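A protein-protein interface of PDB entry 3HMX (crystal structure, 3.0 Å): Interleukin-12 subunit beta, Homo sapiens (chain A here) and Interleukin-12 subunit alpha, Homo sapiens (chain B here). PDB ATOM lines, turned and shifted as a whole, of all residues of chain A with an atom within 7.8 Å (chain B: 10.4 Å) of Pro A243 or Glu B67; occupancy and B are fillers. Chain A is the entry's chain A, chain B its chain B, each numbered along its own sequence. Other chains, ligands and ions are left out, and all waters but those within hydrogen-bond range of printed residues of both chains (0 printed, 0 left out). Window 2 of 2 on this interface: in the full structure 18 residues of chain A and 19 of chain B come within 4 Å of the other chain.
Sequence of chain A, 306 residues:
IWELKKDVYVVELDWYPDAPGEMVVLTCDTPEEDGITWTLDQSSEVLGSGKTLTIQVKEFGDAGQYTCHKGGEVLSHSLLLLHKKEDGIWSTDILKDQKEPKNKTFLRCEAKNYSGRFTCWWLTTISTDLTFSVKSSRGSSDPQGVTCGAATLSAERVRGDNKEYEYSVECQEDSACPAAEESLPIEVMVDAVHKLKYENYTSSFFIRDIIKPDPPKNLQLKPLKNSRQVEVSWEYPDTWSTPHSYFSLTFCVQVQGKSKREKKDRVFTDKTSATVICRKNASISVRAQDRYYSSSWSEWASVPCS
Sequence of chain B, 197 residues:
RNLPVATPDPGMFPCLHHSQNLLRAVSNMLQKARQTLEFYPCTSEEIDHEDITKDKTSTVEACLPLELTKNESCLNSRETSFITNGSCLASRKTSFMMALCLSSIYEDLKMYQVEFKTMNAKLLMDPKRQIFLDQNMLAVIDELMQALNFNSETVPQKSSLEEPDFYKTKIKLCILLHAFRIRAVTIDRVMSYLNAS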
ATOM      1  N   TYR A 236     -32.099  -5.931 -27.150  1.00  0.00           N
ATOM      2  CA  TYR A 236     -31.104  -5.067 -27.796  1.00  0.00           C
ATOM      3  C   TYR A 236     -30.897  -5.423 -29.268  1.00  0.00           C
ATOM      4  O   TYR A 236     -30.800  -6.601 -29.618  1.00  0.00           O
ATOM      5  CB  TYR A 236     -29.764  -5.128 -27.052  1.00  0.00           C
ATOM      6  CG  TYR A 236     -29.636  -4.145 -25.906  1.00  0.00           C
ATOM      7  CD1 TYR A 236     -28.397  -3.638 -25.533  1.00  0.00           C
ATOM      8  CD2 TYR A 236     -30.753  -3.715 -25.205  1.00  0.00           C
ATOM      9  CE1 TYR A 236     -28.274  -2.746 -24.484  1.00  0.00           C
ATOM     10  CE2 TYR A 236     -30.640  -2.817 -24.159  1.00  0.00           C
ATOM     11  CZ  TYR A 236     -29.400  -2.337 -23.802  1.00  0.00           C
ATOM     12  OH  TYR A 236     -29.291  -1.446 -22.756  1.00  0.00           O
ATOM     13  N   TRP A 240     -26.081  -3.468 -32.578  1.00  0.00           N
ATOM     14  CA  TRP A 240     -25.499  -2.754 -31.453  1.00  0.00           C
ATOM     15  C   TRP A 240     -24.285  -3.473 -30.874  1.00  0.00           C
ATOM     16  O   TRP A 240     -24.247  -4.701 -30.805  1.00  0.00           O
ATOM     17  CB  TRP A 240     -26.518  -2.498 -30.351  1.00  0.00           C
ATOM     18  CG  TRP A 240     -25.942  -1.625 -29.292  1.00  0.00           C
ATOM     19  CD1 TRP A 240     -25.491  -2.010 -28.065  1.00  0.00           C
ATOM     20  CD2 TRP A 240     -25.711  -0.216 -29.382  1.00  0.00           C
ATOM     21  NE1 TRP A 240     -25.011  -0.925 -27.375  1.00  0.00           N
ATOM     22  CE2 TRP A 240     -25.135   0.190 -28.161  1.00  0.00           C
ATOM     23  CE3 TRP A 240     -25.944   0.747 -30.373  1.00  0.00           C
ATOM     24  CZ2 TRP A 240     -24.786   1.518 -27.904  1.00  0.00           C
ATOM     25  CZ3 TRP A 240     -25.600   2.063 -30.118  1.00  0.00           C
ATOM     26  CH2 TRP A 240     -25.028   2.437 -28.892  1.00  0.00           C
ATOM     27  N   SER A 241     -23.303  -2.685 -30.448  1.00  0.00           N
ATOM     28  CA  SER A 241     -22.029  -3.208 -29.971  1.00  0.00           C
ATOM     29  C   SER A 241     -22.201  -3.930 -28.627  1.00  0.00           C
ATOM     30  O   SER A 241     -23.066  -3.573 -27.826  1.00  0.00           O
ATOM     31  CB  SER A 241     -21.013  -2.065 -29.858  1.00  0.00           C
ATOM     32  OG  SER A 241     -19.771  -2.410 -30.454  1.00  0.00           O
ATOM     33  N   THR A 242     -21.384  -4.952 -28.394  1.00  0.00           N
ATOM     34  CA  THR A 242     -21.452  -5.736 -27.162  1.00  0.00           C
ATOM     35  C   THR A 242     -20.121  -5.634 -26.417  1.00  0.00           C
ATOM     36  O   THR A 242     -19.098  -5.332 -27.036  1.00  0.00           O
ATOM     37  CB  THR A 242     -21.795  -7.218 -27.462  1.00  0.00           C
ATOM     38  OG1 THR A 242     -20.716  -7.844 -28.170  1.00  0.00           O
ATOM     39  CG2 THR A 242     -23.064  -7.313 -28.299  1.00  0.00           C
ATOM     40  N   PRO A 243     -20.114  -5.880 -25.092  1.00  0.00           N
ATOM     41  CA  PRO A 243     -21.178  -6.297 -24.166  1.00  0.00           C
ATOM     42  C   PRO A 243     -22.167  -5.187 -23.827  1.00  0.00           C
ATOM     43  O   PRO A 243     -21.749  -4.089 -23.473  1.00  0.00           O
ATOM     44  CB  PRO A 243     -20.410  -6.662 -22.888  1.00  0.00           C
ATOM     45  CG  PRO A 243     -18.966  -6.692 -23.263  1.00  0.00           C
ATOM     46  CD  PRO A 243     -18.825  -5.746 -24.398  1.00  0.00           C
ATOM     47  N   HIS A 244     -23.459  -5.491 -23.891  1.00  0.00           N
ATOM     48  CA  HIS A 244     -24.501  -4.493 -23.673  1.00  0.00           C
ATOM     49  C   HIS A 244     -24.380  -3.745 -22.350  1.00  0.00           C
ATOM     50  O   HIS A 244     -25.062  -2.743 -22.141  1.00  0.00           O
ATOM     51  CB  HIS A 244     -25.885  -5.139 -23.758  1.00  0.00           C
ATOM     52  CG  HIS A 244     -26.218  -5.685 -25.110  1.00  0.00           C
ATOM     53  ND1 HIS A 244     -25.810  -5.076 -26.279  1.00  0.00           N
ATOM     54  CD2 HIS A 244     -26.942  -6.766 -25.484  1.00  0.00           C
ATOM     55  CE1 HIS A 244     -26.253  -5.769 -27.313  1.00  0.00           C
ATOM     56  NE2 HIS A 244     -26.946  -6.799 -26.856  1.00  0.00           N
ATOM     57  N   SER A 245     -23.529  -4.235 -21.452  1.00  0.00           N
ATOM     58  CA  SER A 245     -23.370  -3.626 -20.131  1.00  0.00           C
ATOM     59  C   SER A 245     -22.334  -2.515 -20.191  1.00  0.00           C
ATOM     60  O   SER A 245     -22.473  -1.472 -19.550  1.00  0.00           O
ATOM     61  CB  SER A 245     -22.927  -4.673 -19.112  1.00  0.00           C
ATOM     62  OG  SER A 245     -21.581  -5.062 -19.332  1.00  0.00           O
ATOM     63  N   TYR A 246     -21.285  -2.768 -20.963  1.00  0.00           N
ATOM     64  CA  TYR A 246     -20.223  -1.807 -21.190  1.00  0.00           C
ATOM     65  C   TYR A 246     -20.703  -0.784 -22.203  1.00  0.00           C
ATOM     66  O   TYR A 246     -20.159   0.310 -22.308  1.00  0.00           O
ATOM     67  CB  TYR A 246     -18.990  -2.528 -21.726  1.00  0.00           C
ATOM     68  CG  TYR A 246     -17.763  -1.662 -21.823  1.00  0.00           C
ATOM     69  CD1 TYR A 246     -17.393  -1.085 -23.024  1.00  0.00           C
ATOM     70  CD2 TYR A 246     -16.972  -1.421 -20.713  1.00  0.00           C
ATOM     71  CE1 TYR A 246     -16.268  -0.293 -23.121  1.00  0.00           C
ATOM     72  CE2 TYR A 246     -15.843  -0.630 -20.800  1.00  0.00           C
ATOM     73  CZ  TYR A 246     -15.496  -0.070 -22.005  1.00  0.00           C
ATOM     74  OH  TYR A 246     -14.374   0.717 -22.096  1.00  0.00           O
ATOM     75  N   PHE A 247     -21.734  -1.163 -22.951  1.00  0.00           N
ATOM     76  CA  PHE A 247     -22.318  -0.316 -23.980  1.00  0.00           C
ATOM     77  C   PHE A 247     -23.811  -0.179 -23.746  1.00  0.00           C
ATOM     78  O   PHE A 247     -24.617  -0.631 -24.556  1.00  0.00           O
ATOM     79  CB  PHE A 247     -22.100  -0.929 -25.357  1.00  0.00           C
ATOM     80  CG  PHE A 247     -20.666  -0.959 -25.791  1.00  0.00           C
ATOM     81  CD1 PHE A 247     -19.991  -2.158 -25.900  1.00  0.00           C
ATOM     82  CD2 PHE A 247     -19.997   0.209 -26.105  1.00  0.00           C
ATOM     83  CE1 PHE A 247     -18.675  -2.190 -26.311  1.00  0.00           C
ATOM     84  CE2 PHE A 247     -18.681   0.180 -26.512  1.00  0.00           C
ATOM     85  CZ  PHE A 247     -18.020  -1.019 -26.615  1.00  0.00           C
ATOM     86  N   SER A 248     -24.176   0.445 -22.636  1.00  0.00           N
ATOM     87  CA  SER A 248     -25.576   0.564 -22.245  1.00  0.00           C
ATOM     88  C   SER A 248     -26.408   1.286 -23.300  1.00  0.00           C
ATOM     89  O   SER A 248     -25.876   2.059 -24.096  1.00  0.00           O
ATOM     90  CB  SER A 248     -25.677   1.306 -20.917  1.00  0.00           C
ATOM     91  OG  SER A 248     -24.562   1.019 -20.089  1.00  0.00           O
ATOM     92  N   CYS B  63      -8.888  -0.142 -20.923  1.00  0.00           N
ATOM     93  CA  CYS B  63     -10.095  -0.098 -20.105  1.00  0.00           C
ATOM     94  C   CYS B  63     -11.307  -0.685 -20.820  1.00  0.00           C
ATOM     95  O   CYS B  63     -12.443  -0.477 -20.399  1.00  0.00           O
ATOM     96  CB  CYS B  63     -10.394   1.326 -19.648  1.00  0.00           C
ATOM     97  SG  CYS B  63      -9.597   1.783 -18.102  1.00  0.00           S
ATOM     98  N   LEU B  64     -11.061  -1.417 -21.902  1.00  0.00           N
ATOM     99  CA  LEU B  64     -12.135  -2.084 -22.626  1.00  0.00           C
ATOM    100  C   LEU B  64     -12.344  -3.464 -22.026  1.00  0.00           C
ATOM    101  O   LEU B  64     -11.414  -4.037 -21.464  1.00  0.00           O
ATOM    102  CB  LEU B  64     -11.792  -2.219 -24.111  1.00  0.00           C
ATOM    103  CG  LEU B  64     -10.860  -1.188 -24.745  1.00  0.00           C
ATOM    104  CD1 LEU B  64      -9.410  -1.580 -24.492  1.00  0.00           C
ATOM    105  CD2 LEU B  64     -11.128  -1.077 -26.238  1.00  0.00           C
ATOM    106  N   PRO B  65     -13.568  -4.006 -22.142  1.00  0.00           N
ATOM    107  CA  PRO B  65     -13.878  -5.329 -21.590  1.00  0.00           C
ATOM    108  C   PRO B  65     -12.813  -6.354 -21.945  1.00  0.00           C
ATOM    109  O   PRO B  65     -12.058  -6.153 -22.892  1.00  0.00           O
ATOM    110  CB  PRO B  65     -15.198  -5.683 -22.274  1.00  0.00           C
ATOM    111  CG  PRO B  65     -15.851  -4.373 -22.501  1.00  0.00           C
ATOM    112  CD  PRO B  65     -14.745  -3.385 -22.773  1.00  0.00           C
ATOM    113  N   LEU B  66     -12.742  -7.438 -21.184  1.00  0.00           N
ATOM    114  CA  LEU B  66     -11.805  -8.506 -21.500  1.00  0.00           C
ATOM    115  C   LEU B  66     -12.258  -9.202 -22.774  1.00  0.00           C
ATOM    116  O   LEU B  66     -11.486  -9.903 -23.424  1.00  0.00           O
ATOM    117  CB  LEU B  66     -11.713  -9.507 -20.349  1.00  0.00           C
ATOM    118  CG  LEU B  66     -10.956  -9.040 -19.106  1.00  0.00           C
ATOM    119  CD1 LEU B  66     -11.620  -7.815 -18.494  1.00  0.00           C
ATOM    120  CD2 LEU B  66     -10.859 -10.162 -18.088  1.00  0.00           C
ATOM    121  N   GLU B  67     -13.522  -8.991 -23.123  1.00  0.00           N
ATOM    122  CA  GLU B  67     -14.103  -9.585 -24.313  1.00  0.00           C
ATOM    123  C   GLU B  67     -13.495  -9.003 -25.590  1.00  0.00           C
ATOM    124  O   GLU B  67     -13.261  -9.721 -26.562  1.00  0.00           O
ATOM    125  CB  GLU B  67     -15.617  -9.378 -24.307  1.00  0.00           C
ATOM    126  CG  GLU B  67     -16.358 -10.256 -25.290  1.00  0.00           C
ATOM    127  CD  GLU B  67     -17.809  -9.850 -25.454  1.00  0.00           C
ATOM    128  OE1 GLU B  67     -18.103  -8.644 -25.335  1.00  0.00           O
ATOM    129  OE2 GLU B  67     -18.653 -10.736 -25.707  1.00  0.00           O
ATOM    130  N   LEU B  68     -13.238  -7.701 -25.582  1.00  0.00           N
ATOM    131  CA  LEU B  68     -12.688  -7.019 -26.749  1.00  0.00           C
ATOM    132  C   LEU B  68     -11.166  -7.075 -26.746  1.00  0.00           C
ATOM    133  O   LEU B  68     -10.542  -7.249 -27.790  1.00  0.00           O
ATOM    134  CB  LEU B  68     -13.168  -5.570 -26.791  1.00  0.00           C
ATOM    135  CG  LEU B  68     -14.682  -5.425 -26.638  1.00  0.00           C
ATOM    136  CD1 LEU B  68     -15.091  -3.975 -26.744  1.00  0.00           C
ATOM    137  CD2 LEU B  68     -15.408  -6.261 -27.676  1.00  0.00           C
ATOM    138  N   THR B  69     -10.573  -6.921 -25.569  1.00  0.00           N
ATOM    139  CA  THR B  69      -9.146  -7.151 -25.406  1.00  0.00           C
ATOM    140  C   THR B  69      -8.901  -8.655 -25.464  1.00  0.00           C
ATOM    141  O   THR B  69      -8.603  -9.287 -24.447  1.00  0.00           O
ATOM    142  CB  THR B  69      -8.625  -6.597 -24.063  1.00  0.00           C
ATOM    143  OG1 THR B  69      -9.054  -5.240 -23.902  1.00  0.00           O
ATOM    144  CG2 THR B  69      -7.106  -6.648 -24.013  1.00  0.00           C
ATOM    145  N   LYS B  70      -9.050  -9.223 -26.659  1.00  0.00           N
ATOM    146  CA  LYS B  70      -8.870 -10.657 -26.872  1.00  0.00           C
ATOM    147  C   LYS B  70      -7.576 -11.169 -26.240  1.00  0.00           C
ATOM    148  O   LYS B  70      -7.519 -12.297 -25.750  1.00  0.00           O
ATOM    149  CB  LYS B  70      -8.910 -10.983 -28.371  1.00  0.00           C
ATOM    150  CG  LYS B  70      -8.132 -10.012 -29.256  1.00  0.00           C
ATOM    151  CD  LYS B  70      -6.637 -10.294 -29.232  1.00  0.00           C
ATOM    152  CE  LYS B  70      -5.873  -9.363 -30.159  1.00  0.00           C
ATOM    153  NZ  LYS B  70      -6.211  -9.600 -31.589  1.00  0.00           N
ATOM    154  N   ASN B  71      -6.548 -10.324 -26.254  1.00  0.00           N
ATOM    155  CA  ASN B  71      -5.259 -10.625 -25.636  1.00  0.00           C
ATOM    156  C   ASN B  71      -4.430  -9.350 -25.469  1.00  0.00           C
ATOM    157  O   ASN B  71      -4.735  -8.322 -26.073  1.00  0.00           O
ATOM    158  CB  ASN B  71      -4.485 -11.660 -26.455  1.00  0.00           C
ATOM    159  CG  ASN B  71      -4.809 -13.091 -26.054  1.00  0.00           C
ATOM    160  OD1 ASN B  71      -4.735 -14.011 -26.872  1.00  0.00           O
ATOM    161  ND2 ASN B  71      -5.167 -13.287 -24.791  1.00  0.00           N
ATOM    162  N   GLU B  72      -3.385  -9.421 -24.648  1.00  0.00           N
ATOM    163  CA  GLU B  72      -2.533  -8.263 -24.390  1.00  0.00           C
ATOM    164  C   GLU B  72      -1.630  -7.940 -25.578  1.00  0.00           C
ATOM    165  O   GLU B  72      -0.423  -7.754 -25.419  1.00  0.00           O
ATOM    166  CB  GLU B  72      -1.685  -8.490 -23.135  1.00  0.00           C
ATOM    167  N   LYS B  93     -14.052 -10.603 -11.831  1.00  0.00           N
ATOM    168  CA  LYS B  93     -13.568 -10.127 -13.125  1.00  0.00           C
ATOM    169  C   LYS B  93     -12.786  -8.806 -13.061  1.00  0.00           C
ATOM    170  O   LYS B  93     -12.170  -8.406 -14.047  1.00  0.00           O
ATOM    171  CB  LYS B  93     -14.736  -9.986 -14.106  1.00  0.00           C
ATOM    172  N   PHE B  96      -9.001  -8.965 -12.452  1.00  0.00           N
ATOM    173  CA  PHE B  96      -8.441  -9.498 -13.687  1.00  0.00           C
ATOM    174  C   PHE B  96      -7.513  -8.494 -14.368  1.00  0.00           C
ATOM    175  O   PHE B  96      -6.924  -7.636 -13.713  1.00  0.00           O
ATOM    176  CB  PHE B  96      -9.572  -9.894 -14.639  1.00  0.00           C
ATOM    177  CG  PHE B  96      -9.406 -11.253 -15.257  1.00  0.00           C
ATOM    178  CD1 PHE B  96     -10.259 -12.289 -14.917  1.00  0.00           C
ATOM    179  CD2 PHE B  96      -8.402 -11.495 -16.181  1.00  0.00           C
ATOM    180  CE1 PHE B  96     -10.116 -13.540 -15.486  1.00  0.00           C
ATOM    181  CE2 PHE B  96      -8.254 -12.746 -16.752  1.00  0.00           C
ATOM    182  CZ  PHE B  96      -9.112 -13.771 -16.405  1.00  0.00           C
ATOM    183  N   MET B  97      -7.394  -8.608 -15.687  1.00  0.00           N
ATOM    184  CA  MET B  97      -6.522  -7.734 -16.468  1.00  0.00           C
ATOM    185  C   MET B  97      -6.797  -6.253 -16.209  1.00  0.00           C
ATOM    186  O   MET B  97      -5.958  -5.399 -16.496  1.00  0.00           O
ATOM    187  CB  MET B  97      -6.671  -8.024 -17.969  1.00  0.00           C
ATOM    188  CG  MET B  97      -6.165  -9.387 -18.420  1.00  0.00           C
ATOM    189  SD  MET B  97      -6.329  -9.617 -20.205  1.00  0.00           S
ATOM    190  CE  MET B  97      -5.700 -11.282 -20.400  1.00  0.00           C
ATOM    191  N   MET B  98      -7.972  -5.953 -15.666  1.00  0.00           N
ATOM    192  CA  MET B  98      -8.392  -4.570 -15.478  1.00  0.00           C
ATOM    193  C   MET B  98      -7.610  -3.862 -14.380  1.00  0.00           C
ATOM    194  O   MET B  98      -7.837  -2.686 -14.110  1.00  0.00           O
ATOM    195  CB  MET B  98      -9.889  -4.505 -15.183  1.00  0.00           C
ATOM    196  CG  MET B  98     -10.734  -5.297 -16.156  1.00  0.00           C
ATOM    197  SD  MET B  98     -12.387  -4.611 -16.340  1.00  0.00           S
ATOM    198  CE  MET B  98     -12.018  -3.111 -17.247  1.00  0.00           C
ATOM    199  N   ASP B 188     -18.078   5.044 -15.933  1.00  0.00           N
ATOM    200  CA  ASP B 188     -19.350   4.352 -15.782  1.00  0.00           C
ATOM    201  C   ASP B 188     -19.375   3.060 -16.604  1.00  0.00           C
ATOM    202  O   ASP B 188     -19.851   2.028 -16.126  1.00  0.00           O
ATOM    203  CB  ASP B 188     -20.509   5.273 -16.161  1.00  0.00           C
ATOM    204  CG  ASP B 188     -21.817   4.870 -15.510  1.00  0.00           C
ATOM    205  OD1 ASP B 188     -22.423   5.731 -14.841  1.00  0.00           O
ATOM    206  OD2 ASP B 188     -22.236   3.702 -15.663  1.00  0.00           O
ATOM    207  N   ARG B 189     -18.849   3.116 -17.827  1.00  0.00           N
ATOM    208  CA  ARG B 189     -18.766   1.934 -18.687  1.00  0.00           C
ATOM    209  C   ARG B 189     -18.089   0.755 -17.996  1.00  0.00           C
ATOM    210  O   ARG B 189     -18.549  -0.380 -18.097  1.00  0.00           O
ATOM    211  CB  ARG B 189     -18.020   2.255 -19.983  1.00  0.00           C
ATOM    212  CG  ARG B 189     -18.883   2.894 -21.045  1.00  0.00           C
ATOM    213  CD  ARG B 189     -18.269   2.752 -22.434  1.00  0.00           C
ATOM    214  NE  ARG B 189     -19.298   2.865 -23.461  1.00  0.00           N
ATOM    215  CZ  ARG B 189     -19.701   4.013 -23.989  1.00  0.00           C
ATOM    216  NH1 ARG B 189     -19.150   5.152 -23.602  1.00  0.00           N
ATOM    217  NH2 ARG B 189     -20.654   4.025 -24.912  1.00  0.00           N
ATOM    218  N   VAL B 190     -16.988   1.029 -17.306  1.00  0.00           N
ATOM    219  CA  VAL B 190     -16.265  -0.012 -16.592  1.00  0.00           C
ATOM    220  C   VAL B 190     -17.090  -0.511 -15.413  1.00  0.00           C
ATOM    221  O   VAL B 190     -17.298  -1.710 -15.252  1.00  0.00           O
ATOM    222  CB  VAL B 190     -14.906   0.494 -16.084  1.00  0.00           C
ATOM    223  CG1 VAL B 190     -14.186  -0.597 -15.312  1.00  0.00           C
ATOM    224  CG2 VAL B 190     -14.056   0.981 -17.254  1.00  0.00           C
ATOM    225  N   SER B 192     -20.232  -0.320 -14.917  1.00  0.00           N
ATOM    226  CA  SER B 192     -21.426  -1.013 -15.392  1.00  0.00           C
ATOM    227  C   SER B 192     -21.058  -2.413 -15.829  1.00  0.00           C
ATOM    228  O   SER B 192     -21.839  -3.353 -15.682  1.00  0.00           O
ATOM    229  CB  SER B 192     -22.067  -0.265 -16.556  1.00  0.00           C
ATOM    230  OG  SER B 192     -22.663   0.941 -16.110  1.00  0.00           O
ATOM    231  N   TYR B 193     -19.851  -2.538 -16.363  1.00  0.00           N
ATOM    232  CA  TYR B 193     -19.348  -3.809 -16.855  1.00  0.00           C
ATOM    233  C   TYR B 193     -19.077  -4.770 -15.708  1.00  0.00           C
ATOM    234  O   TYR B 193     -19.534  -5.912 -15.724  1.00  0.00           O
ATOM    235  CB  TYR B 193     -18.073  -3.573 -17.651  1.00  0.00           C
ATOM    236  CG  TYR B 193     -17.465  -4.823 -18.225  1.00  0.00           C
ATOM    237  CD1 TYR B 193     -18.156  -5.591 -19.154  1.00  0.00           C
ATOM    238  CD2 TYR B 193     -16.192  -5.227 -17.853  1.00  0.00           C
ATOM    239  CE1 TYR B 193     -17.596  -6.734 -19.688  1.00  0.00           C
ATOM    240  CE2 TYR B 193     -15.625  -6.369 -18.381  1.00  0.00           C
ATOM    241  CZ  TYR B 193     -16.330  -7.117 -19.297  1.00  0.00           C
ATOM    242  OH  TYR B 193     -15.759  -8.251 -19.821  1.00  0.00           O
ATOM    243  N   LEU B 194     -18.336  -4.299 -14.710  1.00  0.00           N
ATOM    244  CA  LEU B 194     -17.990  -5.128 -13.564  1.00  0.00           C
ATOM    245  C   LEU B 194     -19.235  -5.595 -12.824  1.00  0.00           C
ATOM    246  O   LEU B 194     -19.390  -6.783 -12.553  1.00  0.00           O
ATOM    247  CB  LEU B 194     -17.050  -4.377 -12.623  1.00  0.00           C
ATOM    248  CG  LEU B 194     -15.746  -3.927 -13.290  1.00  0.00           C
ATOM    249  CD1 LEU B 194     -14.882  -3.088 -12.356  1.00  0.00           C
ATOM    250  CD2 LEU B 194     -14.971  -5.128 -13.826  1.00  0.00           C
ATOM    251  N   ALA B 196     -21.974  -6.393 -13.700  1.00  0.00           N
ATOM    252  CA  ALA B 196     -22.683  -7.471 -14.385  1.00  0.00           C
ATOM    253  C   ALA B 196     -21.845  -8.737 -14.534  1.00  0.00           C
ATOM    254  O   ALA B 196     -22.377  -9.802 -14.842  1.00  0.00           O
ATOM    255  CB  ALA B 196     -23.185  -7.004 -15.744  1.00  0.00           C
ATOM    256  N   SER B 197     -20.538  -8.624 -14.322  1.00  0.00           N
ATOM    257  CA  SER B 197     -19.655  -9.784 -14.433  1.00  0.00           C
ATOM    258  C   SER B 197     -18.382  -9.655 -13.600  1.00  0.00           C
ATOM    259  O   SER B 197     -17.614  -8.706 -13.739  1.00  0.00           O
ATOM    260  CB  SER B 197     -19.300 -10.050 -15.900  1.00  0.00           C
ATOM    261  OG  SER B 197     -20.353 -10.724 -16.571  1.00  0.00           O
ATOM    262  OXT SER B 197     -18.089 -10.519 -12.776  1.00  0.00           O
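Thr A242 touches Glu B67. Thr A242 touches Leu B68. CG of Pro B65 touches CD of Pro A243, at 3.8 Å. Pro A243 touches Tyr B193. Ser B192 touches Ser A245. OG of Ser A245 touches CD1 of Tyr B193, 3.5 Å away. Tyr A246 touches Leu B64. CG of Tyr A246 touches CG of Pro B65, 3.4 Å away. Tyr A246 touches Tyr B193. CD2 of Phe A247 touches NE of Arg B189, 3.8 Å away.
NE1 of Trp A240 lies within hydrogen-bond range of O of Phe A247, at 2.9 Å. The side-chain hydroxyl (OG) of Ser A248 is in hydrogen-bond range of the backbone carbonyl oxygen (O) of Ser A245, 3.3 Å away. The backbone carbonyl oxygen of Pro B65 sits at hydrogen-bond distance from the side-chain hydroxyl of Thr B69 (3.3 Å). The backbone NH of Leu B66 sits at hydrogen-bond distance from the side-chain hydroxyl of Tyr B193 (3.4 Å). The side-chain hydroxyl (OG) of Ser B192 is in hydrogen-bond range of the side-chain carboxylate (OD2) of Asp B188, at 2.8 Å.
Printed residues of chain B that touch a printed residue of chain A: Cys B63, Leu B64, Pro B65, Glu B67, Leu B68, Arg B189, Ser B192 and Tyr B193. Along chain B the printed residues that touch a printed residue of chain A span positions 63 to 193. Hydrophobic or aromatic side chains of chain A that line the printed part of chain B: Pro A243, Tyr A246 and Phe A247. Among the printed residues, no Asp or Glu carboxylate lies within 4 Å of a Lys or Arg side-chain nitrogen of the other chain.
Of chain A, only Thr A242 (3.8 Å) and Pro A243 (3.0 Å) come within 4 Å of Glu B67. Of chain B, only Glu B67 and Leu B68 come within 4 Å of Thr A242. His A244 touches none of the printed residues of chain B. Ser A245 touches just these residues of chain B: Ser B192 and Tyr B193. Printed residues of chain A within 4 Å of Arg B189: Tyr A246 (2.9 Å) and Phe A247 (3.8 Å). Of the printed residues of chain A, Ser B192 touches Ser A245 (3.3 Å). Ala B196 touches none of the printed residues of chain A.
The side-chain hydroxyl of Tyr A246 is in hydrogen-bond range of the backbone carbonyl oxygen of Cys B63, 2.8 Å away. The guanidinium group (NE) of Arg B189 lies within hydrogen-bond range of the backbone carbonyl oxygen (O) of Tyr A246 (2.9 Å). The backbone nitrogen of Pro A243 lies close to the side-chain carboxylate of Glu B67 (3.4 Å).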
